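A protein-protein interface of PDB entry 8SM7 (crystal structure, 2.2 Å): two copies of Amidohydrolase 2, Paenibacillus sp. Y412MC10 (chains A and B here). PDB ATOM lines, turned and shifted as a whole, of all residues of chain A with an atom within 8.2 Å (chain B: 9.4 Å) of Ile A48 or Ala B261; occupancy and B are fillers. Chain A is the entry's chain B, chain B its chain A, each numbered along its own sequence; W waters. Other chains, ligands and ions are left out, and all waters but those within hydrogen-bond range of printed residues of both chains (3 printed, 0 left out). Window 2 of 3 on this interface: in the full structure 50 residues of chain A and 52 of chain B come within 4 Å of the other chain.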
ATOM      1  N   TYR A  45       7.807  28.178  15.209  1.00  0.00           N
ATOM      2  CA  TYR A  45       6.412  27.898  14.895  1.00  0.00           C
ATOM      3  C   TYR A  45       6.196  27.660  13.397  1.00  0.00           C
ATOM      4  O   TYR A  45       6.238  28.606  12.600  1.00  0.00           O
ATOM      5  CB  TYR A  45       5.554  29.079  15.392  1.00  0.00           C
ATOM      6  CG  TYR A  45       4.092  29.027  15.012  1.00  0.00           C
ATOM      7  CD1 TYR A  45       3.642  29.583  13.816  1.00  0.00           C
ATOM      8  CD2 TYR A  45       3.159  28.441  15.863  1.00  0.00           C
ATOM      9  CE1 TYR A  45       2.300  29.524  13.459  1.00  0.00           C
ATOM     10  CE2 TYR A  45       1.819  28.380  15.523  1.00  0.00           C
ATOM     11  CZ  TYR A  45       1.388  28.926  14.323  1.00  0.00           C
ATOM     12  OH  TYR A  45       0.046  28.858  13.999  1.00  0.00           O
ATOM     13  N   SER A  46       5.972  26.382  12.992  1.00  0.00           N
ATOM     14  CA  SER A  46       5.450  26.148  11.641  1.00  0.00           C
ATOM     15  C   SER A  46       3.921  26.184  11.662  1.00  0.00           C
ATOM     16  O   SER A  46       3.307  25.544  12.526  1.00  0.00           O
ATOM     17  CB  SER A  46       5.925  24.809  11.092  1.00  0.00           C
ATOM     18  OG  SER A  46       5.068  24.354  10.051  1.00  0.00           O
ATOM     19  N   PRO A  47       3.268  26.901  10.732  1.00  0.00           N
ATOM     20  CA  PRO A  47       1.809  27.077  10.822  1.00  0.00           C
ATOM     21  C   PRO A  47       1.038  25.957  10.149  1.00  0.00           C
ATOM     22  O   PRO A  47      -0.102  25.658  10.517  1.00  0.00           O
ATOM     23  CB  PRO A  47       1.585  28.408  10.103  1.00  0.00           C
ATOM     24  CG  PRO A  47       2.627  28.363   9.004  1.00  0.00           C
ATOM     25  CD  PRO A  47       3.824  27.584   9.549  1.00  0.00           C
ATOM     26  N   ILE A  48       1.658  25.337   9.147  1.00  0.00           N
ATOM     27  CA  ILE A  48       1.075  24.198   8.446  1.00  0.00           C
ATOM     28  C   ILE A  48       1.275  22.941   9.283  1.00  0.00           C
ATOM     29  O   ILE A  48       1.317  21.823   8.747  1.00  0.00           O
ATOM     30  CB  ILE A  48       1.706  24.029   7.052  1.00  0.00           C
ATOM     31  CG1 ILE A  48       3.209  23.770   7.189  1.00  0.00           C
ATOM     32  CG2 ILE A  48       1.441  25.264   6.185  1.00  0.00           C
ATOM     33  CD1 ILE A  48       3.934  23.777   5.871  1.00  0.00           C
ATOM     34  N   GLY A  49       1.391  23.118  10.600  1.00  0.00           N
ATOM     35  CA  GLY A  49       1.813  22.048  11.475  1.00  0.00           C
ATOM     36  C   GLY A  49       3.067  21.390  10.937  1.00  0.00           C
ATOM     37  O   GLY A  49       3.880  22.013  10.237  1.00  0.00           O
ATOM     38  N   VAL A  50       3.218  20.100  11.253  1.00  0.00           N
ATOM     39  CA  VAL A  50       4.311  19.279  10.736  1.00  0.00           C
ATOM     40  C   VAL A  50       3.749  18.171   9.839  1.00  0.00           C
ATOM     41  O   VAL A  50       4.403  17.753   8.875  1.00  0.00           O
ATOM     42  CB  VAL A  50       5.168  18.701  11.888  1.00  0.00           C
ATOM     43  CG1 VAL A  50       6.494  18.120  11.365  1.00  0.00           C
ATOM     44  CG2 VAL A  50       5.435  19.769  12.958  1.00  0.00           C
ATOM     45  N   MET A  51       2.526  17.711  10.126  1.00  0.00           N
ATOM     46  CA  MET A  51       1.962  16.529   9.479  1.00  0.00           C
ATOM     47  C   MET A  51       1.151  16.880   8.226  1.00  0.00           C
ATOM     48  O   MET A  51       0.636  17.992   8.071  1.00  0.00           O
ATOM     49  CB  MET A  51       1.084  15.747  10.465  1.00  0.00           C
ATOM     50  CG  MET A  51       1.639  15.657  11.885  1.00  0.00           C
ATOM     51  SD  MET A  51       2.812  14.285  12.125  1.00  0.00           S
ATOM     52  CE  MET A  51       4.323  15.178  12.511  1.00  0.00           C
ATOM     53  N   LYS A  52       1.029  15.892   7.332  1.00  0.00           N
ATOM     54  CA  LYS A  52       0.245  16.035   6.110  1.00  0.00           C
ATOM     55  C   LYS A  52      -1.251  15.876   6.401  1.00  0.00           C
ATOM     56  O   LYS A  52      -1.676  15.651   7.539  1.00  0.00           O
ATOM     57  CB  LYS A  52       0.695  15.018   5.058  1.00  0.00           C
ATOM     58  CG  LYS A  52       0.384  13.566   5.417  1.00  0.00           C
ATOM     59  CD  LYS A  52       1.321  12.586   4.728  1.00  0.00           C
ATOM     60  CE  LYS A  52       0.756  12.113   3.407  1.00  0.00           C
ATOM     61  NZ  LYS A  52      -0.719  11.934   3.498  1.00  0.00           N
ATOM     62  N   LYS A  53      -2.056  15.976   5.337  1.00  0.00           N
ATOM     63  CA  LYS A  53      -3.512  15.871   5.419  1.00  0.00           C
ATOM     64  C   LYS A  53      -3.967  14.413   5.474  1.00  0.00           C
ATOM     65  O   LYS A  53      -3.374  13.536   4.832  1.00  0.00           O
ATOM     66  CB  LYS A  53      -4.151  16.566   4.212  1.00  0.00           C
ATOM     67  N   TYR A 206      10.410  30.333  10.828  1.00  0.00           N
ATOM     68  CA  TYR A 206      10.577  28.922  10.509  1.00  0.00           C
ATOM     69  C   TYR A 206      11.151  28.716   9.112  1.00  0.00           C
ATOM     70  O   TYR A 206      11.980  27.813   8.902  1.00  0.00           O
ATOM     71  CB  TYR A 206       9.234  28.205  10.666  1.00  0.00           C
ATOM     72  CG  TYR A 206       9.190  26.748  10.224  1.00  0.00           C
ATOM     73  CD1 TYR A 206       9.605  25.719  11.072  1.00  0.00           C
ATOM     74  CD2 TYR A 206       8.692  26.398   8.981  1.00  0.00           C
ATOM     75  CE1 TYR A 206       9.539  24.402  10.681  1.00  0.00           C
ATOM     76  CE2 TYR A 206       8.635  25.084   8.577  1.00  0.00           C
ATOM     77  CZ  TYR A 206       9.058  24.086   9.429  1.00  0.00           C
ATOM     78  OH  TYR A 206       8.984  22.776   9.012  1.00  0.00           O
ATOM     79  N   ILE A 207      10.732  29.536   8.139  1.00  0.00           N
ATOM     80  CA  ILE A 207      11.140  29.271   6.758  1.00  0.00           C
ATOM     81  C   ILE A 207      12.647  29.414   6.609  1.00  0.00           C
ATOM     82  O   ILE A 207      13.269  28.666   5.851  1.00  0.00           O
ATOM     83  CB  ILE A 207      10.381  30.164   5.750  1.00  0.00           C
ATOM     84  CG1 ILE A 207      10.724  29.712   4.325  1.00  0.00           C
ATOM     85  CG2 ILE A 207      10.723  31.616   5.919  1.00  0.00           C
ATOM     86  CD1 ILE A 207      10.174  30.572   3.216  1.00  0.00           C
ATOM     87  N   PRO A 317       4.504  11.008   8.171  1.00  0.00           N
ATOM     88  CA  PRO A 317       3.441  11.755   7.496  1.00  0.00           C
ATOM     89  C   PRO A 317       3.619  13.273   7.611  1.00  0.00           C
ATOM     90  O   PRO A 317       2.673  13.963   7.997  1.00  0.00           O
ATOM     91  CB  PRO A 317       2.201  11.313   8.265  1.00  0.00           C
ATOM     92  CG  PRO A 317       2.735  11.175   9.727  1.00  0.00           C
ATOM     93  CD  PRO A 317       4.268  10.992   9.626  1.00  0.00           C
ATOM     94  N   HIS A 318       4.807  13.783   7.303  1.00  0.00           N
ATOM     95  CA  HIS A 318       5.076  15.205   7.449  1.00  0.00           C
ATOM     96  C   HIS A 318       4.616  15.976   6.212  1.00  0.00           C
ATOM     97  O   HIS A 318       4.369  15.401   5.144  1.00  0.00           O
ATOM     98  CB  HIS A 318       6.563  15.450   7.714  1.00  0.00           C
ATOM     99  CG  HIS A 318       6.998  15.059   9.093  1.00  0.00           C
ATOM    100  ND1 HIS A 318       8.322  14.927   9.453  1.00  0.00           N
ATOM    101  CD2 HIS A 318       6.276  14.760  10.199  1.00  0.00           C
ATOM    102  CE1 HIS A 318       8.397  14.578  10.725  1.00  0.00           C
ATOM    103  NE2 HIS A 318       7.169  14.462  11.199  1.00  0.00           N
ATOM    104  N   TRP A 319       4.519  17.307   6.371  1.00  0.00           N
ATOM    105  CA  TRP A 319       3.887  18.149   5.352  1.00  0.00           C
ATOM    106  C   TRP A 319       4.611  18.075   4.010  1.00  0.00           C
ATOM    107  O   TRP A 319       3.969  18.181   2.956  1.00  0.00           O
ATOM    108  CB  TRP A 319       3.783  19.609   5.834  1.00  0.00           C
ATOM    109  CG  TRP A 319       5.081  20.284   6.301  1.00  0.00           C
ATOM    110  CD1 TRP A 319       5.631  20.243   7.560  1.00  0.00           C
ATOM    111  CD2 TRP A 319       5.949  21.120   5.517  1.00  0.00           C
ATOM    112  NE1 TRP A 319       6.792  20.989   7.598  1.00  0.00           N
ATOM    113  CE2 TRP A 319       7.009  21.533   6.359  1.00  0.00           C
ATOM    114  CE3 TRP A 319       5.934  21.553   4.186  1.00  0.00           C
ATOM    115  CZ2 TRP A 319       8.042  22.353   5.911  1.00  0.00           C
ATOM    116  CZ3 TRP A 319       6.966  22.369   3.740  1.00  0.00           C
ATOM    117  CH2 TRP A 319       8.003  22.763   4.602  1.00  0.00           C
ATOM    118  N   ASP A 320       5.937  17.897   4.012  1.00  0.00           N
ATOM    119  CA  ASP A 320       6.661  17.738   2.756  1.00  0.00           C
ATOM    120  C   ASP A 320       6.846  16.272   2.374  1.00  0.00           C
ATOM    121  O   ASP A 320       7.842  15.922   1.724  1.00  0.00           O
ATOM    122  CB  ASP A 320       8.002  18.488   2.783  1.00  0.00           C
ATOM    123  CG  ASP A 320       8.763  18.359   4.108  1.00  0.00           C
ATOM    124  OD1 ASP A 320       8.344  17.613   5.038  1.00  0.00           O
ATOM    125  OD2 ASP A 320       9.795  19.061   4.214  1.00  0.00           O
ATOM    126  N   ARG B 254      15.735  24.814  -2.719  1.00  0.00           N
ATOM    127  CA  ARG B 254      15.207  24.546  -1.357  1.00  0.00           C
ATOM    128  C   ARG B 254      14.349  25.732  -0.906  1.00  0.00           C
ATOM    129  O   ARG B 254      13.242  25.511  -0.406  1.00  0.00           O
ATOM    130  CB  ARG B 254      16.347  24.271  -0.374  1.00  0.00           C
ATOM    131  CG  ARG B 254      15.896  23.860   1.019  1.00  0.00           C
ATOM    132  CD  ARG B 254      16.982  23.105   1.761  1.00  0.00           C
ATOM    133  NE  ARG B 254      16.471  21.900   2.391  1.00  0.00           N
ATOM    134  CZ  ARG B 254      16.300  21.754   3.696  1.00  0.00           C
ATOM    135  NH1 ARG B 254      16.612  22.742   4.513  1.00  0.00           N
ATOM    136  NH2 ARG B 254      15.824  20.624   4.183  1.00  0.00           N
ATOM    137  N   LEU B 255      14.864  26.942  -1.082  1.00  0.00           N
ATOM    138  CA  LEU B 255      14.127  28.117  -0.629  1.00  0.00           C
ATOM    139  C   LEU B 255      12.796  28.266  -1.370  1.00  0.00           C
ATOM    140  O   LEU B 255      11.757  28.534  -0.751  1.00  0.00           O
ATOM    141  CB  LEU B 255      14.991  29.364  -0.814  1.00  0.00           C
ATOM    142  CG  LEU B 255      14.674  30.562   0.067  1.00  0.00           C
ATOM    143  CD1 LEU B 255      14.190  30.094   1.413  1.00  0.00           C
ATOM    144  CD2 LEU B 255      15.896  31.423   0.214  1.00  0.00           C
ATOM    145  N   ASP B 256      12.812  28.085  -2.686  1.00  0.00           N
ATOM    146  CA  ASP B 256      11.576  28.287  -3.484  1.00  0.00           C
ATOM    147  C   ASP B 256      10.525  27.258  -3.068  1.00  0.00           C
ATOM    148  O   ASP B 256       9.344  27.614  -2.986  1.00  0.00           O
ATOM    149  CB  ASP B 256      11.864  28.222  -4.981  1.00  0.00           C
ATOM    150  CG  ASP B 256      12.409  29.511  -5.560  1.00  0.00           C
ATOM    151  OD1 ASP B 256      12.567  30.479  -4.798  1.00  0.00           O
ATOM    152  OD2 ASP B 256      12.668  29.528  -6.771  1.00  0.00           O
ATOM    153  N   LYS B 257      10.961  26.032  -2.808  1.00  0.00           N
ATOM    154  CA  LYS B 257      10.020  24.980  -2.436  1.00  0.00           C
ATOM    155  C   LYS B 257       9.379  25.267  -1.086  1.00  0.00           C
ATOM    156  O   LYS B 257       8.166  25.082  -0.915  1.00  0.00           O
ATOM    157  CB  LYS B 257      10.724  23.621  -2.416  1.00  0.00           C
ATOM    158  CG  LYS B 257       9.815  22.471  -2.002  1.00  0.00           C
ATOM    159  CD  LYS B 257      10.256  21.175  -2.646  1.00  0.00           C
ATOM    160  CE  LYS B 257       9.822  19.965  -1.824  1.00  0.00           C
ATOM    161  NZ  LYS B 257       9.756  18.721  -2.643  1.00  0.00           N
ATOM    162  N   ASN B 258      10.180  25.710  -0.113  1.00  0.00           N
ATOM    163  CA  ASN B 258       9.633  26.093   1.182  1.00  0.00           C
ATOM    164  C   ASN B 258       8.738  27.320   1.055  1.00  0.00           C
ATOM    165  O   ASN B 258       7.735  27.442   1.768  1.00  0.00           O
ATOM    166  CB  ASN B 258      10.774  26.367   2.165  1.00  0.00           C
ATOM    167  CG  ASN B 258      11.391  25.079   2.758  1.00  0.00           C
ATOM    168  OD1 ASN B 258      10.773  24.009   2.797  1.00  0.00           O
ATOM    169  ND2 ASN B 258      12.617  25.203   3.244  1.00  0.00           N
ATOM    170  N   TYR B 259       9.117  28.256   0.181  1.00  0.00           N
ATOM    171  CA  TYR B 259       8.310  29.447  -0.049  1.00  0.00           C
ATOM    172  C   TYR B 259       6.897  29.074  -0.476  1.00  0.00           C
ATOM    173  O   TYR B 259       5.912  29.627   0.036  1.00  0.00           O
ATOM    174  CB  TYR B 259       8.965  30.329  -1.112  1.00  0.00           C
ATOM    175  CG  TYR B 259       8.113  31.516  -1.512  1.00  0.00           C
ATOM    176  CD1 TYR B 259       7.910  32.574  -0.631  1.00  0.00           C
ATOM    177  CD2 TYR B 259       7.516  31.588  -2.768  1.00  0.00           C
ATOM    178  CE1 TYR B 259       7.135  33.671  -0.985  1.00  0.00           C
ATOM    179  CE2 TYR B 259       6.739  32.680  -3.130  1.00  0.00           C
ATOM    180  CZ  TYR B 259       6.553  33.718  -2.235  1.00  0.00           C
ATOM    181  OH  TYR B 259       5.776  34.803  -2.576  1.00  0.00           O
ATOM    182  N   LYS B 260       6.780  28.119  -1.404  1.00  0.00           N
ATOM    183  CA  LYS B 260       5.467  27.729  -1.891  1.00  0.00           C
ATOM    184  C   LYS B 260       4.587  27.243  -0.748  1.00  0.00           C
ATOM    185  O   LYS B 260       3.404  27.591  -0.679  1.00  0.00           O
ATOM    186  CB  LYS B 260       5.606  26.669  -2.992  1.00  0.00           C
ATOM    187  CG  LYS B 260       6.168  27.241  -4.317  1.00  0.00           C
ATOM    188  CD  LYS B 260       6.349  26.181  -5.412  1.00  0.00           C
ATOM    189  CE  LYS B 260       6.908  26.782  -6.717  1.00  0.00           C
ATOM    190  NZ  LYS B 260       8.324  26.363  -7.011  1.00  0.00           N
ATOM    191  N   ALA B 261       5.156  26.488   0.190  1.00  0.00           N
ATOM    192  CA  ALA B 261       4.352  25.962   1.288  1.00  0.00           C
ATOM    193  C   ALA B 261       4.163  26.959   2.422  1.00  0.00           C
ATOM    194  O   ALA B 261       3.234  26.797   3.218  1.00  0.00           O
ATOM    195  CB  ALA B 261       4.974  24.683   1.851  1.00  0.00           C
ATOM    196  N   LEU B 262       5.004  27.985   2.516  1.00  0.00           N
ATOM    197  CA  LEU B 262       5.059  28.808   3.716  1.00  0.00           C
ATOM    198  C   LEU B 262       4.842  30.292   3.433  1.00  0.00           C
ATOM    199  O   LEU B 262       5.012  31.113   4.345  1.00  0.00           O
ATOM    200  CB  LEU B 262       6.404  28.591   4.429  1.00  0.00           C
ATOM    201  CG  LEU B 262       6.721  27.141   4.818  1.00  0.00           C
ATOM    202  CD1 LEU B 262       8.164  26.959   5.261  1.00  0.00           C
ATOM    203  CD2 LEU B 262       5.768  26.679   5.910  1.00  0.00           C
ATOM    204  N   ARG B 263       4.428  30.651   2.212  1.00  0.00           N
ATOM    205  CA  ARG B 263       4.360  32.050   1.808  1.00  0.00           C
ATOM    206  C   ARG B 263       3.545  32.911   2.769  1.00  0.00           C
ATOM    207  O   ARG B 263       3.769  34.125   2.850  1.00  0.00           O
ATOM    208  CB  ARG B 263       3.756  32.153   0.408  1.00  0.00           C
ATOM    209  CG  ARG B 263       2.657  31.144   0.162  1.00  0.00           C
ATOM    210  CD  ARG B 263       2.351  31.038  -1.301  1.00  0.00           C
ATOM    211  NE  ARG B 263       2.349  32.356  -1.912  1.00  0.00           N
ATOM    212  CZ  ARG B 263       2.710  32.608  -3.160  1.00  0.00           C
ATOM    213  NH1 ARG B 263       3.098  31.639  -3.978  1.00  0.00           N
ATOM    214  NH2 ARG B 263       2.690  33.862  -3.592  1.00  0.00           N
ATOM    215  N   ALA B 264       2.576  32.324   3.477  1.00  0.00           N
ATOM    216  CA  ALA B 264       1.742  33.142   4.354  1.00  0.00           C
ATOM    217  C   ALA B 264       2.574  33.788   5.458  1.00  0.00           C
ATOM    218  O   ALA B 264       2.323  34.931   5.842  1.00  0.00           O
ATOM    219  CB  ALA B 264       0.601  32.310   4.942  1.00  0.00           C
ATOM    220  N   THR B 265       3.586  33.080   5.962  1.00  0.00           N
ATOM    221  CA  THR B 265       4.465  33.621   6.992  1.00  0.00           C
ATOM    222  C   THR B 265       5.349  34.744   6.476  1.00  0.00           C
ATOM    223  O   THR B 265       6.002  35.419   7.280  1.00  0.00           O
ATOM    224  CB  THR B 265       5.352  32.513   7.567  1.00  0.00           C
ATOM    225  OG1 THR B 265       6.374  32.180   6.617  1.00  0.00           O
ATOM    226  CG2 THR B 265       4.533  31.271   7.863  1.00  0.00           C
ATOM    227  N   VAL B 266       5.472  34.883   5.164  1.00  0.00           N
ATOM    228  CA  VAL B 266       6.433  35.877   4.616  1.00  0.00           C
ATOM    229  C   VAL B 266       5.703  36.662   3.531  1.00  0.00           C
ATOM    230  O   VAL B 266       6.165  36.690   2.391  1.00  0.00           O
ATOM    231  CB  VAL B 266       7.700  35.147   4.125  1.00  0.00           C
ATOM    232  CG1 VAL B 266       7.443  34.203   2.960  1.00  0.00           C
ATOM    233  CG2 VAL B 266       8.857  36.087   3.850  1.00  0.00           C
ATOM    234  N   MET B 272       9.118  34.653  -6.102  1.00  0.00           N
ATOM    235  CA  MET B 272       9.873  33.541  -5.530  1.00  0.00           C
ATOM    236  C   MET B 272      11.182  34.048  -4.922  1.00  0.00           C
ATOM    237  O   MET B 272      11.830  34.938  -5.496  1.00  0.00           O
ATOM    238  CB  MET B 272      10.183  32.483  -6.586  1.00  0.00           C
ATOM    239  CG  MET B 272       9.057  31.502  -6.891  1.00  0.00           C
ATOM    240  SD  MET B 272       9.617  30.504  -8.285  1.00  0.00           S
ATOM    241  CE  MET B 272       8.630  29.036  -8.062  1.00  0.00           C
ATOM    242  N   PRO B 273      11.599  33.519  -3.762  1.00  0.00           N
ATOM    243  CA  PRO B 273      12.942  33.854  -3.242  1.00  0.00           C
ATOM    244  C   PRO B 273      14.048  33.793  -4.283  1.00  0.00           C
ATOM    245  O   PRO B 273      14.896  34.696  -4.328  1.00  0.00           O
ATOM    246  CB  PRO B 273      13.164  32.814  -2.136  1.00  0.00           C
ATOM    247  CG  PRO B 273      11.819  32.356  -1.730  1.00  0.00           C
ATOM    248  CD  PRO B 273      10.806  32.760  -2.785  1.00  0.00           C
HETATM  249  O   HOH W   1       8.154  30.729   8.227  1.00  0.00           O
HETATM  250  O   HOH W   2      10.455  21.195   2.535  1.00  0.00           O
HETATM  251  O   HOH W   3       8.720  17.272  -0.821  1.00  0.00           O
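The guanidinium group (NH2) of Arg B263 is in hydrogen-bond range of the side-chain hydroxyl (OH) of Tyr B259 (3.4 Å).
The backbone carbonyl oxygen of Leu B262 sits at hydrogen-bond distance from the side-chain hydroxyl of Thr B265 (2.9 Å).
The backbone carbonyl oxygen of Val A50 lies within hydrogen-bond range of the backbone NH of Trp A319 (2.5 Å).
The side-chain hydroxyl of Tyr A206 lies within hydrogen-bond range of the indole nitrogen of Trp A319 (3.2 Å).
Water W3 bridges the side-chain amino group of Lys B257 (2.5 Å) and the backbone carbonyl oxygen of Asp A320 (3.0 Å).
Water W2 bridges OD2 of Asp A320 (2.8 Å) and OD1 of Asn B258 (2.8 Å).
Water W1 lies within hydrogen-bond range of OG1 of Thr B265, N of Ile A207 and N of Tyr A206.
No position is printed for both chains.
Of the 9 pairs that touch across the chains among the printed residues, none has its exchanged pair printed and touching as well.
Printed residues of chain B that touch a printed residue of chain A: Asn B258, Tyr B259, Ala B261, Leu B262 and Thr B265.
Hydrophobic or aromatic side chains of chain B that line the printed part of chain A: Ala B261 and Leu B262.
Among the printed residues, 9 pairs touch across the chains.
Of chain B, only Ala B261 and Leu B262 come within 4 Å of Ile A48.
Ala B261 touches just these residues of chain A: Ile A48 and Trp A319.
Of chain B, only Thr B265 (3.7 Å) comes within 4 Å of Pro A47.
Of the printed residues of chain B, Ile A207 touches Asn B258, Tyr B259 and Leu B262.
Of the printed residues of chain A, Tyr B259 touches Ile A207.
Of the printed residues of chain B, Trp A319 touches Asn B258 (3.5 Å) and Ala B261 (3.6 Å).
Of the printed residues of chain B, Tyr A206 touches Leu B262 (3.8 Å).
Of the printed residues of chain A, Thr B265 touches Pro A47.
Pro B273 touches none of the printed residues of chain A.
Ala B264 touches none of the printed residues of chain A.
The nearest residue of chain A that does not touch Ala B261 is Pro A47 (6.0 Å).
The nearest printed residue of chain A that does not touch Asn B258 is Asp A320 (5.2 Å).
Among the printed residues, merely in contact across the chains: Pro A47 with Thr B265 (3.7 Å), Ile A48 with Ala B261 (3.8 Å), Ile A48 with Leu B262 (3.4 Å), Tyr A206 with Leu B262 (3.8 Å), Ile A207 with Asn B258 (3.98 Å), Ile A207 with Tyr B259 (3.9 Å), Ile A207 with Leu B262 (3.9 Å), Trp A319 with Asn B258 (3.5 Å) and Trp A319 with Ala B261 (3.6 Å).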
